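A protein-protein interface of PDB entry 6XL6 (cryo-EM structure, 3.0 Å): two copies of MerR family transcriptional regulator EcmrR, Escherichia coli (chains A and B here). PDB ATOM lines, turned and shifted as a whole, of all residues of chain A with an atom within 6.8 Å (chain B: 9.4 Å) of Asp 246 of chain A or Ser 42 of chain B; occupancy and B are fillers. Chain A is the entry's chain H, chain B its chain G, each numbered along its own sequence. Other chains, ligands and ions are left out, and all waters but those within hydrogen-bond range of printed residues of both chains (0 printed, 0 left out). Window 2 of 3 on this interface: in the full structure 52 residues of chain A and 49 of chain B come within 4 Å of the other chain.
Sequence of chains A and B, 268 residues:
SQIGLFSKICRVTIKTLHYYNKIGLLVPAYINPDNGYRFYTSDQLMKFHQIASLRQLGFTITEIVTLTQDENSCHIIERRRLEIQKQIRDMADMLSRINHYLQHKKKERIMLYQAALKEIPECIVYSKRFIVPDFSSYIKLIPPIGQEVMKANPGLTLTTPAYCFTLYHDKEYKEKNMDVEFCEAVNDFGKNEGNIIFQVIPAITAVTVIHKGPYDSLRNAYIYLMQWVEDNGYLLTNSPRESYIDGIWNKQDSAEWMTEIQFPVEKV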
ATOM      1  N   ILE A 210       2.199   3.673  12.732  1.00  0.00           N
ATOM      2  CA  ILE A 210       1.452   4.756  12.110  1.00  0.00           C
ATOM      3  C   ILE A 210       0.038   4.749  12.667  1.00  0.00           C
ATOM      4  O   ILE A 210      -0.596   3.694  12.763  1.00  0.00           O
ATOM      5  CB  ILE A 210       1.450   4.623  10.582  1.00  0.00           C
ATOM      6  CG1 ILE A 210       2.866   4.766  10.042  1.00  0.00           C
ATOM      7  CG2 ILE A 210       0.603   5.688   9.969  1.00  0.00           C
ATOM      8  CD1 ILE A 210       2.971   4.529   8.567  1.00  0.00           C
ATOM      9  N   LYS A 212      -3.683   6.381  12.233  1.00  0.00           N
ATOM     10  CA  LYS A 212      -4.645   7.112  11.423  1.00  0.00           C
ATOM     11  C   LYS A 212      -5.853   7.434  12.288  1.00  0.00           C
ATOM     12  O   LYS A 212      -6.523   6.524  12.788  1.00  0.00           O
ATOM     13  CB  LYS A 212      -5.056   6.303  10.194  1.00  0.00           C
ATOM     14  CG  LYS A 212      -5.505   7.153   9.023  1.00  0.00           C
ATOM     15  CD  LYS A 212      -5.594   6.338   7.749  1.00  0.00           C
ATOM     16  CE  LYS A 212      -5.717   7.237   6.534  1.00  0.00           C
ATOM     17  NZ  LYS A 212      -5.779   6.457   5.269  1.00  0.00           N
ATOM     18  N   GLY A 213      -6.127   8.723  12.466  1.00  0.00           N
ATOM     19  CA  GLY A 213      -7.223   9.158  13.295  1.00  0.00           C
ATOM     20  C   GLY A 213      -6.925  10.469  13.988  1.00  0.00           C
ATOM     21  O   GLY A 213      -5.951  11.156  13.673  1.00  0.00           O
ATOM     22  N   TYR A 215      -5.920  13.129  17.124  1.00  0.00           N
ATOM     23  CA  TYR A 215      -4.747  13.163  17.987  1.00  0.00           C
ATOM     24  C   TYR A 215      -5.081  12.766  19.417  1.00  0.00           C
ATOM     25  O   TYR A 215      -4.195  12.328  20.157  1.00  0.00           O
ATOM     26  CB  TYR A 215      -4.116  14.550  17.953  1.00  0.00           C
ATOM     27  CG  TYR A 215      -3.353  14.819  16.684  1.00  0.00           C
ATOM     28  CD1 TYR A 215      -2.727  13.790  16.006  1.00  0.00           C
ATOM     29  CD2 TYR A 215      -3.271  16.095  16.158  1.00  0.00           C
ATOM     30  CE1 TYR A 215      -2.032  14.024  14.845  1.00  0.00           C
ATOM     31  CE2 TYR A 215      -2.579  16.338  14.995  1.00  0.00           C
ATOM     32  CZ  TYR A 215      -1.960  15.298  14.343  1.00  0.00           C
ATOM     33  OH  TYR A 215      -1.265  15.531  13.181  1.00  0.00           O
ATOM     34  N   SER A 243       5.962  11.559  14.519  1.00  0.00           N
ATOM     35  CA  SER A 243       6.101  12.188  13.215  1.00  0.00           C
ATOM     36  C   SER A 243       4.731  12.563  12.672  1.00  0.00           C
ATOM     37  O   SER A 243       3.813  11.740  12.668  1.00  0.00           O
ATOM     38  CB  SER A 243       6.821  11.261  12.238  1.00  0.00           C
ATOM     39  OG  SER A 243       6.680  11.723  10.909  1.00  0.00           O
ATOM     40  N   TYR A 244       4.596  13.807  12.222  1.00  0.00           N
ATOM     41  CA  TYR A 244       3.342  14.304  11.665  1.00  0.00           C
ATOM     42  C   TYR A 244       3.426  14.225  10.146  1.00  0.00           C
ATOM     43  O   TYR A 244       4.029  15.063   9.480  1.00  0.00           O
ATOM     44  CB  TYR A 244       3.071  15.719  12.149  1.00  0.00           C
ATOM     45  CG  TYR A 244       3.020  15.831  13.646  1.00  0.00           C
ATOM     46  CD1 TYR A 244       1.912  15.399  14.350  1.00  0.00           C
ATOM     47  CD2 TYR A 244       4.084  16.355  14.355  1.00  0.00           C
ATOM     48  CE1 TYR A 244       1.860  15.494  15.714  1.00  0.00           C
ATOM     49  CE2 TYR A 244       4.043  16.452  15.721  1.00  0.00           C
ATOM     50  CZ  TYR A 244       2.928  16.018  16.397  1.00  0.00           C
ATOM     51  OH  TYR A 244       2.877  16.113  17.765  1.00  0.00           O
ATOM     52  N   ILE A 245       2.804  13.184   9.595  1.00  0.00           N
ATOM     53  CA  ILE A 245       2.820  12.994   8.149  1.00  0.00           C
ATOM     54  C   ILE A 245       1.678  13.763   7.501  1.00  0.00           C
ATOM     55  O   ILE A 245       1.868  14.470   6.506  1.00  0.00           O
ATOM     56  CB  ILE A 245       2.757  11.499   7.805  1.00  0.00           C
ATOM     57  CG1 ILE A 245       3.876  10.743   8.511  1.00  0.00           C
ATOM     58  CG2 ILE A 245       2.880  11.304   6.313  1.00  0.00           C
ATOM     59  CD1 ILE A 245       3.709   9.251   8.465  1.00  0.00           C
ATOM     60  N   ASP A 246       0.477  13.574   8.035  1.00  0.00           N
ATOM     61  CA  ASP A 246      -0.717  14.241   7.530  1.00  0.00           C
ATOM     62  C   ASP A 246      -1.463  14.853   8.700  1.00  0.00           C
ATOM     63  O   ASP A 246      -1.428  14.320   9.808  1.00  0.00           O
ATOM     64  CB  ASP A 246      -1.631  13.247   6.809  1.00  0.00           C
ATOM     65  CG  ASP A 246      -1.457  13.276   5.303  1.00  0.00           C
ATOM     66  OD1 ASP A 246      -0.615  14.054   4.807  1.00  0.00           O
ATOM     67  OD2 ASP A 246      -2.173  12.522   4.612  1.00  0.00           O
ATOM     68  N   GLY A 247      -2.140  15.971   8.465  1.00  0.00           N
ATOM     69  CA  GLY A 247      -2.872  16.599   9.542  1.00  0.00           C
ATOM     70  C   GLY A 247      -3.753  17.703   9.015  1.00  0.00           C
ATOM     71  O   GLY A 247      -4.200  17.665   7.868  1.00  0.00           O
ATOM     72  N   ILE A 248      -4.006  18.692   9.875  1.00  0.00           N
ATOM     73  CA  ILE A 248      -4.909  19.779   9.524  1.00  0.00           C
ATOM     74  C   ILE A 248      -4.358  20.628   8.389  1.00  0.00           C
ATOM     75  O   ILE A 248      -5.117  21.341   7.727  1.00  0.00           O
ATOM     76  CB  ILE A 248      -5.208  20.636  10.771  1.00  0.00           C
ATOM     77  CG1 ILE A 248      -6.561  21.326  10.638  1.00  0.00           C
ATOM     78  CG2 ILE A 248      -4.120  21.666  10.997  1.00  0.00           C
ATOM     79  CD1 ILE A 248      -7.064  21.907  11.934  1.00  0.00           C
ATOM     80  N   TRP A 249      -3.051  20.561   8.135  1.00  0.00           N
ATOM     81  CA  TRP A 249      -2.455  21.338   7.057  1.00  0.00           C
ATOM     82  C   TRP A 249      -2.662  20.713   5.688  1.00  0.00           C
ATOM     83  O   TRP A 249      -2.603  21.431   4.686  1.00  0.00           O
ATOM     84  CB  TRP A 249      -0.958  21.504   7.303  1.00  0.00           C
ATOM     85  CG  TRP A 249      -0.238  20.204   7.341  1.00  0.00           C
ATOM     86  CD1 TRP A 249       0.364  19.568   6.297  1.00  0.00           C
ATOM     87  CD2 TRP A 249      -0.053  19.366   8.483  1.00  0.00           C
ATOM     88  NE1 TRP A 249       0.916  18.385   6.720  1.00  0.00           N
ATOM     89  CE2 TRP A 249       0.672  18.239   8.060  1.00  0.00           C
ATOM     90  CE3 TRP A 249      -0.430  19.462   9.823  1.00  0.00           C
ATOM     91  CZ2 TRP A 249       1.030  17.220   8.928  1.00  0.00           C
ATOM     92  CZ3 TRP A 249      -0.073  18.450  10.681  1.00  0.00           C
ATOM     93  CH2 TRP A 249       0.646  17.343  10.232  1.00  0.00           C
ATOM     94  N   ASN A 250      -2.893  19.405   5.618  1.00  0.00           N
ATOM     95  CA  ASN A 250      -2.921  18.711   4.339  1.00  0.00           C
ATOM     96  C   ASN A 250      -4.299  18.141   4.043  1.00  0.00           C
ATOM     97  O   ASN A 250      -4.640  17.902   2.880  1.00  0.00           O
ATOM     98  CB  ASN A 250      -1.876  17.595   4.326  1.00  0.00           C
ATOM     99  CG  ASN A 250      -1.241  17.409   2.968  1.00  0.00           C
ATOM    100  OD1 ASN A 250      -1.087  18.362   2.205  1.00  0.00           O
ATOM    101  ND2 ASN A 250      -0.865  16.176   2.656  1.00  0.00           N
ATOM    102  N   LYS A 251      -5.099  17.922   5.081  1.00  0.00           N
ATOM    103  CA  LYS A 251      -6.418  17.322   4.937  1.00  0.00           C
ATOM    104  C   LYS A 251      -7.374  17.987   5.910  1.00  0.00           C
ATOM    105  O   LYS A 251      -6.967  18.412   6.995  1.00  0.00           O
ATOM    106  CB  LYS A 251      -6.363  15.811   5.177  1.00  0.00           C
ATOM    107  CG  LYS A 251      -5.789  15.042   4.005  1.00  0.00           C
ATOM    108  CD  LYS A 251      -5.696  13.560   4.282  1.00  0.00           C
ATOM    109  CE  LYS A 251      -5.301  12.815   3.023  1.00  0.00           C
ATOM    110  NZ  LYS A 251      -4.227  13.535   2.288  1.00  0.00           N
ATOM    111  N   GLU A 256      -8.750  11.197   8.617  1.00  0.00           N
ATOM    112  CA  GLU A 256      -7.661  10.835   7.721  1.00  0.00           C
ATOM    113  C   GLU A 256      -6.338  11.463   8.134  1.00  0.00           C
ATOM    114  O   GLU A 256      -5.386  11.446   7.346  1.00  0.00           O
ATOM    115  CB  GLU A 256      -7.996  11.226   6.280  1.00  0.00           C
ATOM    116  CG  GLU A 256      -8.719  10.138   5.507  1.00  0.00           C
ATOM    117  CD  GLU A 256      -9.101  10.570   4.104  1.00  0.00           C
ATOM    118  OE1 GLU A 256      -8.284  11.244   3.442  1.00  0.00           O
ATOM    119  OE2 GLU A 256     -10.218  10.233   3.661  1.00  0.00           O
ATOM    120  N   TRP A 257      -6.255  12.022   9.338  1.00  0.00           N
ATOM    121  CA  TRP A 257      -4.981  12.517   9.834  1.00  0.00           C
ATOM    122  C   TRP A 257      -4.055  11.349  10.124  1.00  0.00           C
ATOM    123  O   TRP A 257      -4.402  10.429  10.868  1.00  0.00           O
ATOM    124  CB  TRP A 257      -5.182  13.348  11.097  1.00  0.00           C
ATOM    125  CG  TRP A 257      -5.801  14.672  10.842  1.00  0.00           C
ATOM    126  CD1 TRP A 257      -5.976  15.270   9.636  1.00  0.00           C
ATOM    127  CD2 TRP A 257      -6.332  15.570  11.819  1.00  0.00           C
ATOM    128  NE1 TRP A 257      -6.582  16.490   9.797  1.00  0.00           N
ATOM    129  CE2 TRP A 257      -6.811  16.696  11.131  1.00  0.00           C
ATOM    130  CE3 TRP A 257      -6.449  15.530  13.209  1.00  0.00           C
ATOM    131  CZ2 TRP A 257      -7.399  17.771  11.781  1.00  0.00           C
ATOM    132  CZ3 TRP A 257      -7.029  16.597  13.853  1.00  0.00           C
ATOM    133  CH2 TRP A 257      -7.498  17.704  13.141  1.00  0.00           C
ATOM    134  N   MET A 258      -2.866  11.387   9.535  1.00  0.00           N
ATOM    135  CA  MET A 258      -1.934  10.279   9.651  1.00  0.00           C
ATOM    136  C   MET A 258      -0.691  10.744  10.389  1.00  0.00           C
ATOM    137  O   MET A 258      -0.010  11.671   9.943  1.00  0.00           O
ATOM    138  CB  MET A 258      -1.565   9.729   8.273  1.00  0.00           C
ATOM    139  CG  MET A 258      -1.114   8.295   8.306  1.00  0.00           C
ATOM    140  SD  MET A 258      -0.952   7.565   6.677  1.00  0.00           S
ATOM    141  CE  MET A 258       0.560   8.348   6.138  1.00  0.00           C
ATOM    142  N   THR A 259      -0.406  10.100  11.516  1.00  0.00           N
ATOM    143  CA  THR A 259       0.756  10.420  12.328  1.00  0.00           C
ATOM    144  C   THR A 259       1.493   9.132  12.658  1.00  0.00           C
ATOM    145  O   THR A 259       0.876   8.075  12.808  1.00  0.00           O
ATOM    146  CB  THR A 259       0.354  11.167  13.606  1.00  0.00           C
ATOM    147  OG1 THR A 259       1.515  11.427  14.403  1.00  0.00           O
ATOM    148  CG2 THR A 259      -0.659  10.377  14.404  1.00  0.00           C
ATOM    149  N   SER B   1       2.286  12.397  -4.423  1.00  0.00           N
ATOM    150  CA  SER B   1       3.650  11.951  -4.172  1.00  0.00           C
ATOM    151  C   SER B   1       4.121  11.019  -5.277  1.00  0.00           C
ATOM    152  O   SER B   1       3.599   9.919  -5.433  1.00  0.00           O
ATOM    153  CB  SER B   1       3.744  11.252  -2.817  1.00  0.00           C
ATOM    154  OG  SER B   1       5.080  11.229  -2.352  1.00  0.00           O
ATOM    155  N   PHE B   6       8.127   8.928  -2.942  1.00  0.00           N
ATOM    156  CA  PHE B   6       7.584   7.857  -2.116  1.00  0.00           C
ATOM    157  C   PHE B   6       8.662   6.857  -1.726  1.00  0.00           C
ATOM    158  O   PHE B   6       8.633   6.303  -0.621  1.00  0.00           O
ATOM    159  CB  PHE B   6       6.448   7.157  -2.849  1.00  0.00           C
ATOM    160  CG  PHE B   6       5.557   6.358  -1.953  1.00  0.00           C
ATOM    161  CD1 PHE B   6       4.772   6.984  -1.008  1.00  0.00           C
ATOM    162  CD2 PHE B   6       5.503   4.983  -2.058  1.00  0.00           C
ATOM    163  CE1 PHE B   6       3.952   6.254  -0.185  1.00  0.00           C
ATOM    164  CE2 PHE B   6       4.682   4.249  -1.237  1.00  0.00           C
ATOM    165  CZ  PHE B   6       3.907   4.885  -0.300  1.00  0.00           C
ATOM    166  N   ILE B   9      10.290   8.468   1.138  1.00  0.00           N
ATOM    167  CA  ILE B   9       9.413   8.427   2.306  1.00  0.00           C
ATOM    168  C   ILE B   9       9.449   7.044   2.937  1.00  0.00           C
ATOM    169  O   ILE B   9       9.580   6.896   4.158  1.00  0.00           O
ATOM    170  CB  ILE B   9       7.981   8.828   1.911  1.00  0.00           C
ATOM    171  CG1 ILE B   9       7.897  10.332   1.659  1.00  0.00           C
ATOM    172  CG2 ILE B   9       6.994   8.413   2.983  1.00  0.00           C
ATOM    173  CD1 ILE B   9       6.514  10.812   1.304  1.00  0.00           C
ATOM    174  N   CYS B  10       9.353   6.007   2.106  1.00  0.00           N
ATOM    175  CA  CYS B  10       9.332   4.635   2.594  1.00  0.00           C
ATOM    176  C   CYS B  10      10.727   4.104   2.889  1.00  0.00           C
ATOM    177  O   CYS B  10      10.851   3.079   3.568  1.00  0.00           O
ATOM    178  CB  CYS B  10       8.643   3.738   1.567  1.00  0.00           C
ATOM    179  SG  CYS B  10       6.857   3.920   1.522  1.00  0.00           S
ATOM    180  N   LEU B  26       1.202  -3.539  -3.617  1.00  0.00           N
ATOM    181  CA  LEU B  26       0.995  -2.116  -3.351  1.00  0.00           C
ATOM    182  C   LEU B  26       0.761  -1.439  -4.700  1.00  0.00           C
ATOM    183  O   LEU B  26       1.682  -1.247  -5.494  1.00  0.00           O
ATOM    184  CB  LEU B  26       2.182  -1.511  -2.607  1.00  0.00           C
ATOM    185  CG  LEU B  26       2.039  -0.079  -2.106  1.00  0.00           C
ATOM    186  CD1 LEU B  26       1.103  -0.038  -0.921  1.00  0.00           C
ATOM    187  CD2 LEU B  26       3.395   0.469  -1.730  1.00  0.00           C
ATOM    188  N   ALA B  29      -2.037   4.980  -6.116  1.00  0.00           N
ATOM    189  CA  ALA B  29      -3.374   5.555  -6.066  1.00  0.00           C
ATOM    190  C   ALA B  29      -3.813   6.062  -7.430  1.00  0.00           C
ATOM    191  O   ALA B  29      -5.006   6.033  -7.746  1.00  0.00           O
ATOM    192  CB  ALA B  29      -3.423   6.681  -5.036  1.00  0.00           C
ATOM    193  N   PHE B  39       1.815   7.542  -9.033  1.00  0.00           N
ATOM    194  CA  PHE B  39       1.652   8.520  -7.971  1.00  0.00           C
ATOM    195  C   PHE B  39       1.067   7.834  -6.748  1.00  0.00           C
ATOM    196  O   PHE B  39       0.194   6.970  -6.869  1.00  0.00           O
ATOM    197  CB  PHE B  39       0.757   9.673  -8.412  1.00  0.00           C
ATOM    198  CG  PHE B  39       1.339  10.491  -9.522  1.00  0.00           C
ATOM    199  CD1 PHE B  39       1.029  10.214 -10.837  1.00  0.00           C
ATOM    200  CD2 PHE B  39       2.201  11.533  -9.249  1.00  0.00           C
ATOM    201  CE1 PHE B  39       1.565  10.962 -11.859  1.00  0.00           C
ATOM    202  CE2 PHE B  39       2.740  12.283 -10.267  1.00  0.00           C
ATOM    203  CZ  PHE B  39       2.420  11.997 -11.573  1.00  0.00           C
ATOM    204  N   TYR B  40       1.549   8.219  -5.576  1.00  0.00           N
ATOM    205  CA  TYR B  40       1.197   7.563  -4.327  1.00  0.00           C
ATOM    206  C   TYR B  40       0.520   8.551  -3.385  1.00  0.00           C
ATOM    207  O   TYR B  40       0.458   9.754  -3.641  1.00  0.00           O
ATOM    208  CB  TYR B  40       2.434   6.939  -3.685  1.00  0.00           C
ATOM    209  CG  TYR B  40       3.001   5.791  -4.481  1.00  0.00           C
ATOM    210  CD1 TYR B  40       3.940   6.009  -5.475  1.00  0.00           C
ATOM    211  CD2 TYR B  40       2.589   4.490  -4.245  1.00  0.00           C
ATOM    212  CE1 TYR B  40       4.457   4.965  -6.202  1.00  0.00           C
ATOM    213  CE2 TYR B  40       3.102   3.441  -4.968  1.00  0.00           C
ATOM    214  CZ  TYR B  40       4.035   3.686  -5.944  1.00  0.00           C
ATOM    215  OH  TYR B  40       4.545   2.640  -6.667  1.00  0.00           O
ATOM    216  N   THR B  41       0.004   8.019  -2.281  1.00  0.00           N
ATOM    217  CA  THR B  41      -0.834   8.775  -1.366  1.00  0.00           C
ATOM    218  C   THR B  41      -0.569   8.232   0.034  1.00  0.00           C
ATOM    219  O   THR B  41      -0.003   7.149   0.194  1.00  0.00           O
ATOM    220  CB  THR B  41      -2.311   8.662  -1.802  1.00  0.00           C
ATOM    221  OG1 THR B  41      -2.459   9.259  -3.094  1.00  0.00           O
ATOM    222  CG2 THR B  41      -3.272   9.383  -0.863  1.00  0.00           C
ATOM    223  N   SER B  42      -0.943   9.017   1.050  1.00  0.00           N
ATOM    224  CA  SER B  42      -0.758   8.622   2.443  1.00  0.00           C
ATOM    225  C   SER B  42      -1.316   7.234   2.735  1.00  0.00           C
ATOM    226  O   SER B  42      -0.734   6.474   3.517  1.00  0.00           O
ATOM    227  CB  SER B  42      -1.419   9.653   3.350  1.00  0.00           C
ATOM    228  OG  SER B  42      -0.832  10.927   3.162  1.00  0.00           O
ATOM    229  N   ASP B  43      -2.444   6.884   2.121  1.00  0.00           N
ATOM    230  CA  ASP B  43      -2.997   5.549   2.294  1.00  0.00           C
ATOM    231  C   ASP B  43      -2.160   4.464   1.628  1.00  0.00           C
ATOM    232  O   ASP B  43      -2.374   3.282   1.913  1.00  0.00           O
ATOM    233  CB  ASP B  43      -4.443   5.503   1.785  1.00  0.00           C
ATOM    234  CG  ASP B  43      -4.592   6.014   0.362  1.00  0.00           C
ATOM    235  OD1 ASP B  43      -3.620   5.962  -0.416  1.00  0.00           O
ATOM    236  OD2 ASP B  43      -5.700   6.476   0.019  1.00  0.00           O
ATOM    237  N   GLN B  44      -1.223   4.828   0.751  1.00  0.00           N
ATOM    238  CA  GLN B  44      -0.267   3.846   0.252  1.00  0.00           C
ATOM    239  C   GLN B  44       0.890   3.668   1.225  1.00  0.00           C
ATOM    240  O   GLN B  44       1.436   2.569   1.347  1.00  0.00           O
ATOM    241  CB  GLN B  44       0.255   4.260  -1.122  1.00  0.00           C
ATOM    242  CG  GLN B  44      -0.807   4.811  -2.046  1.00  0.00           C
ATOM    243  CD  GLN B  44      -1.822   3.770  -2.437  1.00  0.00           C
ATOM    244  OE1 GLN B  44      -2.993   3.858  -2.075  1.00  0.00           O
ATOM    245  NE2 GLN B  44      -1.378   2.769  -3.180  1.00  0.00           N
ATOM    246  N   LEU B  45       1.276   4.737   1.921  1.00  0.00           N
ATOM    247  CA  LEU B  45       2.281   4.611   2.970  1.00  0.00           C
ATOM    248  C   LEU B  45       1.748   3.791   4.135  1.00  0.00           C
ATOM    249  O   LEU B  45       2.475   2.976   4.717  1.00  0.00           O
ATOM    250  CB  LEU B  45       2.717   5.996   3.442  1.00  0.00           C
ATOM    251  CG  LEU B  45       3.659   6.039   4.639  1.00  0.00           C
ATOM    252  CD1 LEU B  45       4.950   5.319   4.313  1.00  0.00           C
ATOM    253  CD2 LEU B  45       3.936   7.469   5.040  1.00  0.00           C
ATOM    254  N   MET B  46       0.472   3.986   4.475  1.00  0.00           N
ATOM    255  CA  MET B  46      -0.157   3.197   5.526  1.00  0.00           C
ATOM    256  C   MET B  46      -0.169   1.713   5.185  1.00  0.00           C
ATOM    257  O   MET B  46      -0.178   0.869   6.087  1.00  0.00           O
ATOM    258  CB  MET B  46      -1.578   3.713   5.764  1.00  0.00           C
ATOM    259  CG  MET B  46      -2.344   3.039   6.884  1.00  0.00           C
ATOM    260  SD  MET B  46      -1.669   3.375   8.513  1.00  0.00           S
ATOM    261  CE  MET B  46      -3.035   2.879   9.554  1.00  0.00           C
ATOM    262  N   LYS B  47      -0.148   1.370   3.894  1.00  0.00           N
ATOM    263  CA  LYS B  47      -0.149  -0.035   3.504  1.00  0.00           C
ATOM    264  C   LYS B  47       1.265  -0.580   3.348  1.00  0.00           C
ATOM    265  O   LYS B  47       1.515  -1.752   3.646  1.00  0.00           O
ATOM    266  CB  LYS B  47      -0.937  -0.228   2.210  1.00  0.00           C
ATOM    267  CG  LYS B  47      -1.067  -1.683   1.795  1.00  0.00           C
ATOM    268  CD  LYS B  47      -2.238  -1.907   0.868  1.00  0.00           C
ATOM    269  CE  LYS B  47      -2.444  -3.388   0.611  1.00  0.00           C
ATOM    270  NZ  LYS B  47      -3.613  -3.642  -0.274  1.00  0.00           N
ATOM    271  N   PHE B  48       2.201   0.247   2.880  1.00  0.00           N
ATOM    272  CA  PHE B  48       3.591  -0.191   2.840  1.00  0.00           C
ATOM    273  C   PHE B  48       4.121  -0.432   4.244  1.00  0.00           C
ATOM    274  O   PHE B  48       4.988  -1.288   4.448  1.00  0.00           O
ATOM    275  CB  PHE B  48       4.467   0.826   2.115  1.00  0.00           C
ATOM    276  CG  PHE B  48       5.900   0.396   1.992  1.00  0.00           C
ATOM    277  CD1 PHE B  48       6.842   0.793   2.923  1.00  0.00           C
ATOM    278  CD2 PHE B  48       6.301  -0.417   0.953  1.00  0.00           C
ATOM    279  CE1 PHE B  48       8.154   0.393   2.814  1.00  0.00           C
ATOM    280  CE2 PHE B  48       7.610  -0.818   0.840  1.00  0.00           C
ATOM    281  CZ  PHE B  48       8.538  -0.412   1.771  1.00  0.00           C
ATOM    282  N   HIS B  49       3.618   0.315   5.225  1.00  0.00           N
ATOM    283  CA  HIS B  49       3.997   0.042   6.604  1.00  0.00           C
ATOM    284  C   HIS B  49       3.538  -1.345   7.032  1.00  0.00           C
ATOM    285  O   HIS B  49       4.268  -2.059   7.724  1.00  0.00           O
ATOM    286  CB  HIS B  49       3.421   1.105   7.529  1.00  0.00           C
ATOM    287  CG  HIS B  49       4.103   1.176   8.855  1.00  0.00           C
ATOM    288  ND1 HIS B  49       3.583   0.595   9.990  1.00  0.00           N
ATOM    289  CD2 HIS B  49       5.270   1.752   9.226  1.00  0.00           C
ATOM    290  CE1 HIS B  49       4.399   0.811  11.004  1.00  0.00           C
ATOM    291  NE2 HIS B  49       5.429   1.512  10.568  1.00  0.00           N
ATOM    292  N   GLN B  50       2.340  -1.754   6.609  1.00  0.00           N
ATOM    293  CA  GLN B  50       1.869  -3.102   6.909  1.00  0.00           C
ATOM    294  C   GLN B  50       2.700  -4.149   6.181  1.00  0.00           C
ATOM    295  O   GLN B  50       3.025  -5.200   6.747  1.00  0.00           O
ATOM    296  CB  GLN B  50       0.397  -3.235   6.531  1.00  0.00           C
ATOM    297  CG  GLN B  50      -0.165  -4.627   6.733  1.00  0.00           C
ATOM    298  CD  GLN B  50      -1.665  -4.678   6.565  1.00  0.00           C
ATOM    299  OE1 GLN B  50      -2.305  -5.673   6.900  1.00  0.00           O
ATOM    300  NE2 GLN B  50      -2.237  -3.603   6.041  1.00  0.00           N
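Met 46 of chain B touches Ile 210 of chain A (SD to CG2, 3.6 Å).
CG of His 49 of chain B touches CD1 of Ile 210 of chain A, at 3.6 Å.
Lys 212 of chain A touches Asp 43 of chain B (NZ to CB, 3.9 Å).
Ile 245 of chain A touches Leu 45 of chain B (CD1 to CD2, 3.9 Å).
CD2 of Leu 45 of chain B touches CE of Met 258 of chain A, 3.7 Å away.
Hydrophobic or aromatic side chains of chain B within 4 Å of the printed part of chain A: Leu 45, Met 46 and His 49.
Of the 17 printed residues of chain A, 5 touch a printed residue of chain B.
Along chain A the printed residues that touch a printed residue of chain B span positions 210 to 258.
Among the printed residues, no Asp or Glu carboxylate lies within 4 Å of a Lys or Arg side-chain nitrogen of the other chain.
The side-chain carboxylate of Asp 43 of chain B sits close to the side-chain amide oxygen of Gln 44 of chain B (2.8 Å).
The backbone carbonyl oxygen (O) of Met 258 of chain A is in hydrogen-bond range of the backbone NH (N) of Ile 245 of chain A (3.2 Å).
The side-chain amide nitrogen (ND2) of Asn 250 of chain A sits at hydrogen-bond distance from the side-chain carboxylate (OD1) of Asp 246 of chain A.
The side-chain amino group (NZ) of Lys 251 of chain A lies within salt-bridge range of the side-chain carboxylate (OD2) of Asp 246 of chain A.
The backbone carbonyl oxygen (O) of Met 258 of chain A sits at hydrogen-bond distance from the backbone NH (N) of Asp 246 of chain A.
The side-chain hydroxyl (OG) of Ser 42 of chain B sits at hydrogen-bond distance from the side-chain carboxylate (OD2) of Asp 246 of chain A, at 2.5 Å.
The backbone carbonyl oxygen (O) of Ser 42 of chain B sits close to the side-chain sulfur (SD) of Met 258 of chain A.
No position is printed for both chains.
Of the 7 pairs that touch across the chains among the printed residues, none has its exchanged pair printed and touching as well.
Asp 246 of chain A touches just one residue of chain B: Ser 42.
Of the printed residues of chain A, Ser 42 of chain B touches Asp 246 and Met 258.
No residue of chain B comes within 4 Å of Gly 247 of chain A.
Of the printed residues of chain B, Ile 245 of chain A touches Leu 45 (3.9 Å).
Of the printed residues of chain B, Ile 210 of chain A touches Met 46 (3.6 Å) and His 49 (3.6 Å).
Tyr 40 of chain B touches none of the printed residues of chain A.
The nearest residue of chain B that does not touch Asp 246 of chain A is Asp 43 of chain B (6.2 Å).
The nearest printed residue of chain A that does not touch His 49 of chain B is Ile 245 of chain A (7.7 Å).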
